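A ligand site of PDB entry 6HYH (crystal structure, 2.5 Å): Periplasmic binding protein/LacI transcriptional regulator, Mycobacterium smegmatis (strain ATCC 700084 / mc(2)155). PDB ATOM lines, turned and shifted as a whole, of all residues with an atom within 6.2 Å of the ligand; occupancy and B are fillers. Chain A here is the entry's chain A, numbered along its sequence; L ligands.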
ATOM      1  N   GLU A  27     -16.290  -0.897   2.588  1.00  0.00           N
ATOM      2  CA  GLU A  27     -15.515  -0.048   3.482  1.00  0.00           C
ATOM      3  C   GLU A  27     -14.542  -0.840   4.364  1.00  0.00           C
ATOM      4  O   GLU A  27     -13.545  -0.289   4.828  1.00  0.00           O
ATOM      5  CB  GLU A  27     -16.455   0.793   4.360  1.00  0.00           C
ATOM      6  CG  GLU A  27     -17.456   0.030   5.245  1.00  0.00           C
ATOM      7  CD  GLU A  27     -18.601  -0.639   4.454  1.00  0.00           C
ATOM      8  OE1 GLU A  27     -19.314  -1.544   5.032  1.00  0.00           O
ATOM      9  OE2 GLU A  27     -18.747  -0.239   3.242  1.00  0.00           O
ATOM     10  N   SER A  28     -14.811  -2.133   4.602  1.00  0.00           N
ATOM     11  CA  SER A  28     -14.127  -2.893   5.636  1.00  0.00           C
ATOM     12  C   SER A  28     -13.949  -4.347   5.213  1.00  0.00           C
ATOM     13  O   SER A  28     -14.655  -4.863   4.327  1.00  0.00           O
ATOM     14  CB  SER A  28     -14.897  -2.839   6.970  1.00  0.00           C
ATOM     15  OG  SER A  28     -15.959  -3.789   6.950  1.00  0.00           O
ATOM     16  N   GLY A  29     -13.021  -5.032   5.877  1.00  0.00           N
ATOM     17  CA  GLY A  29     -12.864  -6.439   5.590  1.00  0.00           C
ATOM     18  C   GLY A  29     -14.099  -7.229   5.938  1.00  0.00           C
ATOM     19  O   GLY A  29     -14.450  -8.191   5.241  1.00  0.00           O
ATOM     20  N   TRP A  30     -14.826  -6.814   6.985  1.00  0.00           N
ATOM     21  CA  TRP A  30     -16.098  -7.480   7.234  1.00  0.00           C
ATOM     22  C   TRP A  30     -17.021  -7.324   6.032  1.00  0.00           C
ATOM     23  O   TRP A  30     -17.640  -8.299   5.597  1.00  0.00           O
ATOM     24  CB  TRP A  30     -16.758  -6.904   8.482  1.00  0.00           C
ATOM     25  CG  TRP A  30     -17.973  -7.650   8.970  1.00  0.00           C
ATOM     26  CD1 TRP A  30     -18.066  -8.366  10.122  1.00  0.00           C
ATOM     27  CD2 TRP A  30     -19.271  -7.676   8.365  1.00  0.00           C
ATOM     28  NE1 TRP A  30     -19.362  -8.860  10.282  1.00  0.00           N
ATOM     29  CE2 TRP A  30     -20.122  -8.449   9.215  1.00  0.00           C
ATOM     30  CE3 TRP A  30     -19.827  -7.115   7.211  1.00  0.00           C
ATOM     31  CZ2 TRP A  30     -21.455  -8.693   8.930  1.00  0.00           C
ATOM     32  CZ3 TRP A  30     -21.173  -7.361   6.930  1.00  0.00           C
ATOM     33  CH2 TRP A  30     -21.967  -8.142   7.787  1.00  0.00           C
ATOM     34  N   ARG A  31     -17.143  -6.112   5.474  1.00  0.00           N
ATOM     35  CA  ARG A  31     -18.118  -5.935   4.400  1.00  0.00           C
ATOM     36  C   ARG A  31     -17.722  -6.743   3.175  1.00  0.00           C
ATOM     37  O   ARG A  31     -18.574  -7.392   2.559  1.00  0.00           O
ATOM     38  CB  ARG A  31     -18.227  -4.458   4.026  1.00  0.00           C
ATOM     39  CG  ARG A  31     -19.271  -4.117   2.957  1.00  0.00           C
ATOM     40  CD  ARG A  31     -20.659  -4.435   3.425  1.00  0.00           C
ATOM     41  NE  ARG A  31     -20.876  -3.864   4.754  1.00  0.00           N
ATOM     42  CZ  ARG A  31     -21.966  -4.079   5.477  1.00  0.00           C
ATOM     43  NH1 ARG A  31     -22.080  -3.533   6.691  1.00  0.00           N
ATOM     44  NH2 ARG A  31     -22.947  -4.837   4.994  1.00  0.00           N
ATOM     45  N   SER A  79     -28.759  -4.036   2.828  1.00  0.00           N
ATOM     46  CA  SER A  79     -28.231  -3.746   4.153  1.00  0.00           C
ATOM     47  C   SER A  79     -28.139  -2.238   4.278  1.00  0.00           C
ATOM     48  O   SER A  79     -27.209  -1.632   3.704  1.00  0.00           O
ATOM     49  CB  SER A  79     -26.874  -4.423   4.306  1.00  0.00           C
ATOM     50  OG  SER A  79     -25.996  -3.674   5.115  1.00  0.00           O
ATOM     51  N   ASP A 104     -28.103  -7.540   8.178  1.00  0.00           N
ATOM     52  CA  ASP A 104     -27.066  -6.977   9.061  1.00  0.00           C
ATOM     53  C   ASP A 104     -27.498  -5.669   9.710  1.00  0.00           C
ATOM     54  O   ASP A 104     -27.489  -5.584  10.939  1.00  0.00           O
ATOM     55  CB  ASP A 104     -25.667  -6.886   8.403  1.00  0.00           C
ATOM     56  CG  ASP A 104     -25.385  -5.575   7.700  1.00  0.00           C
ATOM     57  OD1 ASP A 104     -26.332  -4.964   7.188  1.00  0.00           O
ATOM     58  OD2 ASP A 104     -24.202  -5.141   7.712  1.00  0.00           O
ATOM     59  N   ARG A 105     -27.911  -4.647   8.941  1.00  0.00           N
ATOM     60  CA  ARG A 105     -28.208  -3.330   9.492  1.00  0.00           C
ATOM     61  C   ARG A 105     -29.715  -3.066   9.497  1.00  0.00           C
ATOM     62  O   ARG A 105     -30.428  -3.467   8.579  1.00  0.00           O
ATOM     63  CB  ARG A 105     -27.490  -2.220   8.705  1.00  0.00           C
ATOM     64  CG  ARG A 105     -25.997  -2.230   8.872  1.00  0.00           C
ATOM     65  CD  ARG A 105     -25.343  -0.962   8.342  1.00  0.00           C
ATOM     66  NE  ARG A 105     -23.886  -1.109   8.316  1.00  0.00           N
ATOM     67  CZ  ARG A 105     -23.045  -0.195   7.827  1.00  0.00           C
ATOM     68  NH1 ARG A 105     -23.487   0.939   7.326  1.00  0.00           N
ATOM     69  NH2 ARG A 105     -21.732  -0.411   7.858  1.00  0.00           N
ATOM     70  N   ALA A 121     -26.623  -9.511  13.338  1.00  0.00           N
ATOM     71  CA  ALA A 121     -26.015  -9.715  14.638  1.00  0.00           C
ATOM     72  C   ALA A 121     -26.661  -8.779  15.661  1.00  0.00           C
ATOM     73  O   ALA A 121     -27.393  -7.851  15.300  1.00  0.00           O
ATOM     74  CB  ALA A 121     -24.503  -9.461  14.556  1.00  0.00           C
ATOM     75  N   PHE A 123     -25.805  -5.987  17.691  1.00  0.00           N
ATOM     76  CA  PHE A 123     -24.733  -4.990  17.829  1.00  0.00           C
ATOM     77  C   PHE A 123     -24.641  -4.415  19.231  1.00  0.00           C
ATOM     78  O   PHE A 123     -23.531  -4.104  19.711  1.00  0.00           O
ATOM     79  CB  PHE A 123     -24.988  -3.867  16.843  1.00  0.00           C
ATOM     80  CG  PHE A 123     -25.086  -4.337  15.444  1.00  0.00           C
ATOM     81  CD1 PHE A 123     -24.076  -5.134  14.921  1.00  0.00           C
ATOM     82  CD2 PHE A 123     -26.146  -3.965  14.646  1.00  0.00           C
ATOM     83  CE1 PHE A 123     -24.123  -5.569  13.620  1.00  0.00           C
ATOM     84  CE2 PHE A 123     -26.212  -4.377  13.347  1.00  0.00           C
ATOM     85  CZ  PHE A 123     -25.192  -5.186  12.823  1.00  0.00           C
ATOM     86  N   GLU A 126     -22.592  -6.719  21.295  1.00  0.00           N
ATOM     87  CA  GLU A 126     -21.177  -6.665  20.944  1.00  0.00           C
ATOM     88  C   GLU A 126     -20.508  -5.502  21.662  1.00  0.00           C
ATOM     89  O   GLU A 126     -19.445  -5.667  22.301  1.00  0.00           O
ATOM     90  CB  GLU A 126     -21.006  -6.541  19.425  1.00  0.00           C
ATOM     91  CG  GLU A 126     -21.527  -7.719  18.592  1.00  0.00           C
ATOM     92  CD  GLU A 126     -21.558  -7.394  17.069  1.00  0.00           C
ATOM     93  OE1 GLU A 126     -21.215  -6.232  16.702  1.00  0.00           O
ATOM     94  OE2 GLU A 126     -21.901  -8.295  16.247  1.00  0.00           O
ATOM     95  N   THR A 153     -19.764   4.752  10.887  1.00  0.00           N
ATOM     96  CA  THR A 153     -20.490   5.678   9.999  1.00  0.00           C
ATOM     97  C   THR A 153     -21.647   6.288  10.769  1.00  0.00           C
ATOM     98  O   THR A 153     -22.576   5.569  11.136  1.00  0.00           O
ATOM     99  CB  THR A 153     -21.020   4.947   8.750  1.00  0.00           C
ATOM    100  OG1 THR A 153     -19.968   4.183   8.115  1.00  0.00           O
ATOM    101  CG2 THR A 153     -21.622   5.920   7.748  1.00  0.00           C
ATOM    102  N   PRO A 158     -25.170  -0.423  13.323  1.00  0.00           N
ATOM    103  CA  PRO A 158     -24.109  -0.965  14.193  1.00  0.00           C
ATOM    104  C   PRO A 158     -23.358   0.083  15.009  1.00  0.00           C
ATOM    105  O   PRO A 158     -23.044  -0.155  16.183  1.00  0.00           O
ATOM    106  CB  PRO A 158     -23.164  -1.681  13.206  1.00  0.00           C
ATOM    107  CG  PRO A 158     -23.597  -1.221  11.790  1.00  0.00           C
ATOM    108  CD  PRO A 158     -25.073  -0.942  11.931  1.00  0.00           C
ATOM    109  N   ARG A 162     -23.493  -0.120  18.938  1.00  0.00           N
ATOM    110  CA  ARG A 162     -22.251  -0.478  19.601  1.00  0.00           C
ATOM    111  C   ARG A 162     -21.842   0.595  20.591  1.00  0.00           C
ATOM    112  O   ARG A 162     -21.435   0.272  21.717  1.00  0.00           O
ATOM    113  CB  ARG A 162     -21.164  -0.721  18.553  1.00  0.00           C
ATOM    114  CG  ARG A 162     -21.376  -1.986  17.763  1.00  0.00           C
ATOM    115  CD  ARG A 162     -20.193  -2.306  16.844  1.00  0.00           C
ATOM    116  NE  ARG A 162     -20.492  -3.463  15.997  1.00  0.00           N
ATOM    117  CZ  ARG A 162     -19.995  -3.632  14.763  1.00  0.00           C
ATOM    118  NH1 ARG A 162     -19.178  -2.726  14.234  1.00  0.00           N
ATOM    119  NH2 ARG A 162     -20.330  -4.710  14.062  1.00  0.00           N
ATOM    120  N   ASP A 185     -15.806   6.243  10.113  1.00  0.00           N
ATOM    121  CA  ASP A 185     -16.452   5.689   8.910  1.00  0.00           C
ATOM    122  C   ASP A 185     -16.135   4.218   8.666  1.00  0.00           C
ATOM    123  O   ASP A 185     -16.201   3.757   7.518  1.00  0.00           O
ATOM    124  CB  ASP A 185     -16.072   6.484   7.675  1.00  0.00           C
ATOM    125  CG  ASP A 185     -17.070   7.519   7.344  1.00  0.00           C
ATOM    126  OD1 ASP A 185     -18.251   7.149   7.120  1.00  0.00           O
ATOM    127  OD2 ASP A 185     -16.656   8.705   7.343  1.00  0.00           O
ATOM    128  N   PHE A 186     -15.892   3.458   9.721  1.00  0.00           N
ATOM    129  CA  PHE A 186     -15.643   2.014   9.604  1.00  0.00           C
ATOM    130  C   PHE A 186     -14.494   1.706   8.625  1.00  0.00           C
ATOM    131  O   PHE A 186     -14.482   0.657   7.971  1.00  0.00           O
ATOM    132  CB  PHE A 186     -16.915   1.279   9.155  1.00  0.00           C
ATOM    133  CG  PHE A 186     -17.901   1.050  10.235  1.00  0.00           C
ATOM    134  CD1 PHE A 186     -17.504   0.680  11.504  1.00  0.00           C
ATOM    135  CD2 PHE A 186     -19.263   1.185   9.982  1.00  0.00           C
ATOM    136  CE1 PHE A 186     -18.475   0.450  12.527  1.00  0.00           C
ATOM    137  CE2 PHE A 186     -20.214   0.955  10.979  1.00  0.00           C
ATOM    138  CZ  PHE A 186     -19.815   0.595  12.257  1.00  0.00           C
ATOM    139  N   GLN A 211     -14.960   0.484  16.919  1.00  0.00           N
ATOM    140  CA  GLN A 211     -16.279  -0.061  16.613  1.00  0.00           C
ATOM    141  C   GLN A 211     -16.233  -1.085  15.490  1.00  0.00           C
ATOM    142  O   GLN A 211     -17.125  -1.935  15.413  1.00  0.00           O
ATOM    143  CB  GLN A 211     -17.278   1.058  16.275  1.00  0.00           C
ATOM    144  CG  GLN A 211     -17.682   1.860  17.498  1.00  0.00           C
ATOM    145  CD  GLN A 211     -18.889   2.679  17.236  1.00  0.00           C
ATOM    146  OE1 GLN A 211     -19.467   2.616  16.153  1.00  0.00           O
ATOM    147  NE2 GLN A 211     -19.307   3.457  18.230  1.00  0.00           N
ATOM    148  N   ASN A 212     -15.246  -0.998  14.603  1.00  0.00           N
ATOM    149  CA  ASN A 212     -14.919  -2.132  13.761  1.00  0.00           C
ATOM    150  C   ASN A 212     -13.417  -2.280  13.768  1.00  0.00           C
ATOM    151  O   ASN A 212     -12.693  -1.292  13.958  1.00  0.00           O
ATOM    152  CB  ASN A 212     -15.519  -2.013  12.339  1.00  0.00           C
ATOM    153  CG  ASN A 212     -14.725  -1.124  11.393  1.00  0.00           C
ATOM    154  OD1 ASN A 212     -13.956  -0.243  11.800  1.00  0.00           O
ATOM    155  ND2 ASN A 212     -14.904  -1.364  10.089  1.00  0.00           N
ATOM    156  N   ASP A 213     -12.930  -3.516  13.651  1.00  0.00           N
ATOM    157  CA  ASP A 213     -11.502  -3.634  13.900  1.00  0.00           C
ATOM    158  C   ASP A 213     -10.673  -3.105  12.737  1.00  0.00           C
ATOM    159  O   ASP A 213      -9.465  -2.929  12.903  1.00  0.00           O
ATOM    160  CB  ASP A 213     -11.145  -5.066  14.347  1.00  0.00           C
ATOM    161  CG  ASP A 213     -11.519  -6.138  13.369  1.00  0.00           C
ATOM    162  OD1 ASP A 213     -11.529  -5.809  12.160  1.00  0.00           O
ATOM    163  OD2 ASP A 213     -11.793  -7.294  13.810  1.00  0.00           O
ATOM    164  N   ASP A 214     -11.299  -2.745  11.620  1.00  0.00           N
ATOM    165  CA  ASP A 214     -10.569  -1.995  10.600  1.00  0.00           C
ATOM    166  C   ASP A 214     -10.115  -0.639  11.130  1.00  0.00           C
ATOM    167  O   ASP A 214      -8.947  -0.242  10.960  1.00  0.00           O
ATOM    168  CB  ASP A 214     -11.457  -1.828   9.375  1.00  0.00           C
ATOM    169  CG  ASP A 214     -11.332  -2.982   8.413  1.00  0.00           C
ATOM    170  OD1 ASP A 214     -10.249  -3.143   7.834  1.00  0.00           O
ATOM    171  OD2 ASP A 214     -12.309  -3.762   8.287  1.00  0.00           O
ATOM    172  N   VAL A 239     -14.544  -4.662  17.468  1.00  0.00           N
ATOM    173  CA  VAL A 239     -15.640  -5.538  17.037  1.00  0.00           C
ATOM    174  C   VAL A 239     -15.417  -5.966  15.589  1.00  0.00           C
ATOM    175  O   VAL A 239     -14.943  -5.160  14.772  1.00  0.00           O
ATOM    176  CB  VAL A 239     -16.994  -4.854  17.211  1.00  0.00           C
ATOM    177  CG1 VAL A 239     -18.084  -5.810  16.804  1.00  0.00           C
ATOM    178  CG2 VAL A 239     -17.164  -4.410  18.661  1.00  0.00           C
ATOM    179  N   ASP A 240     -15.742  -7.232  15.291  1.00  0.00           N
ATOM    180  CA  ASP A 240     -15.727  -7.880  13.968  1.00  0.00           C
ATOM    181  C   ASP A 240     -15.015  -9.243  13.993  1.00  0.00           C
ATOM    182  O   ASP A 240     -15.621 -10.283  13.714  1.00  0.00           O
ATOM    183  CB  ASP A 240     -15.113  -7.010  12.861  1.00  0.00           C
ATOM    184  CG  ASP A 240     -16.138  -6.085  12.219  1.00  0.00           C
ATOM    185  OD1 ASP A 240     -17.326  -6.147  12.632  1.00  0.00           O
ATOM    186  OD2 ASP A 240     -15.759  -5.296  11.316  1.00  0.00           O
ATOM    187  N   THR A 242     -12.383  -9.807  12.004  1.00  0.00           N
ATOM    188  CA  THR A 242     -11.983  -9.971  10.614  1.00  0.00           C
ATOM    189  C   THR A 242     -10.702 -10.787  10.532  1.00  0.00           C
ATOM    190  O   THR A 242     -10.083 -11.110  11.553  1.00  0.00           O
ATOM    191  CB  THR A 242     -11.741  -8.616   9.979  1.00  0.00           C
ATOM    192  OG1 THR A 242     -10.670  -7.976  10.691  1.00  0.00           O
ATOM    193  CG2 THR A 242     -13.013  -7.747  10.065  1.00  0.00           C
ATOM    194  N   CYS A 260     -18.161 -10.577  14.845  1.00  0.00           N
ATOM    195  CA  CYS A 260     -19.396 -10.321  14.123  1.00  0.00           C
ATOM    196  C   CYS A 260     -19.322 -11.116  12.833  1.00  0.00           C
ATOM    197  O   CYS A 260     -18.330 -11.037  12.104  1.00  0.00           O
ATOM    198  CB  CYS A 260     -19.589  -8.826  13.814  1.00  0.00           C
ATOM    199  SG  CYS A 260     -21.251  -8.456  13.111  1.00  0.00           S
HETATM  200  O1  LIG L   1     -18.973  -4.056  11.778  1.00  0.00           O
HETATM  201  C1  LIG L   1     -18.185  -3.005   9.681  1.00  0.00           C
HETATM  202  C2  LIG L   1     -18.897  -2.748   8.356  1.00  0.00           C
HETATM  203  O2  LIG L   1     -22.781  -3.439   9.528  1.00  0.00           O
HETATM  204  C3  LIG L   1     -21.953  -4.882  11.350  1.00  0.00           C
HETATM  205  O3  LIG L   1     -20.285  -2.868   8.656  1.00  0.00           O
HETATM  206  C4  LIG L   1     -21.702  -4.260   9.984  1.00  0.00           C
HETATM  207  C5  LIG L   1     -20.478  -3.357   9.986  1.00  0.00           C
HETATM  208  C6  LIG L   1     -19.142  -3.985  10.369  1.00  0.00           C
HETATM  209  O4  LIG L   1     -18.639  -1.486   7.800  1.00  0.00           O
HETATM  210  O5  LIG L   1     -16.905  -3.616   9.562  1.00  0.00           O
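An oxygen (O5) of the ligand sits at hydrogen-bond distance from the side-chain carboxylate (OD2) of Asp 240, 2.7 Å away. NH2 of Arg 162 lies within hydrogen-bond range of O1 of the ligand (2.7 Å). An oxygen (O3) of the ligand lies within hydrogen-bond range of the guanidinium group (NH1) of Arg 31 (2.7 Å). The side-chain hydroxyl of Ser 28 is in hydrogen-bond range of an oxygen (O5) of the ligand (2.8 Å). The guanidinium group of Arg 105 lies within hydrogen-bond range of an oxygen (O2) of the ligand (2.8 Å). An oxygen (O4) of the ligand is in hydrogen-bond range of the side-chain carboxylate (OE1) of Glu 27 (2.8 Å). The side-chain carboxylate (OD2) of Asp 104 is in hydrogen-bond range of an oxygen (O2) of the ligand, 2.9 Å away. An oxygen (O5) of the ligand lies within hydrogen-bond range of the side-chain amide nitrogen (ND2) of Asn 212, at 3.1 Å.
The side-chain carboxylate (OD1) of Asp 240 lies within salt-bridge range of the guanidinium group (NH2) of Arg 162 (3.6 Å). NE of Arg 162 lies within salt-bridge range of OE1 of Glu 126 (2.9 Å). The guanidinium group (NE) of Arg 31 lies within salt-bridge range of the side-chain carboxylate (OE1) of Glu 27 (2.8 Å). The side-chain hydroxyl (OG) of Ser 79 is in hydrogen-bond range of the guanidinium group (NH2) of Arg 31 (3.3 Å). The backbone NH of Trp 30 lies close to the side-chain hydroxyl of Ser 28 (3.2 Å). The guanidinium group of Arg 105 lies within salt-bridge range of the side-chain carboxylate of Glu 27, 3.9 Å away. The side-chain carboxylate (OD1) of Asp 104 is in hydrogen-bond range of the side-chain hydroxyl (OG) of Ser 79. The indole nitrogen (NE1) of Trp 30 sits at hydrogen-bond distance from the backbone carbonyl oxygen (O) of Cys 260 (3.0 Å).
Merely in contact with the ligand: Phe 123 (3.2 Å), Pro 158 (3.3 Å), Trp 30 (3.5 Å) and Phe 186 (3.5 Å). Hydrophobic or aromatic side chains within 4 Å of the ligand: Trp 30, Phe 123, Pro 158 and Phe 186. Of the 24 residues printed, 12 come within 4 Å of the ligand. Along chain A the residues within 4 Å of the ligand span positions 27 to 240.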
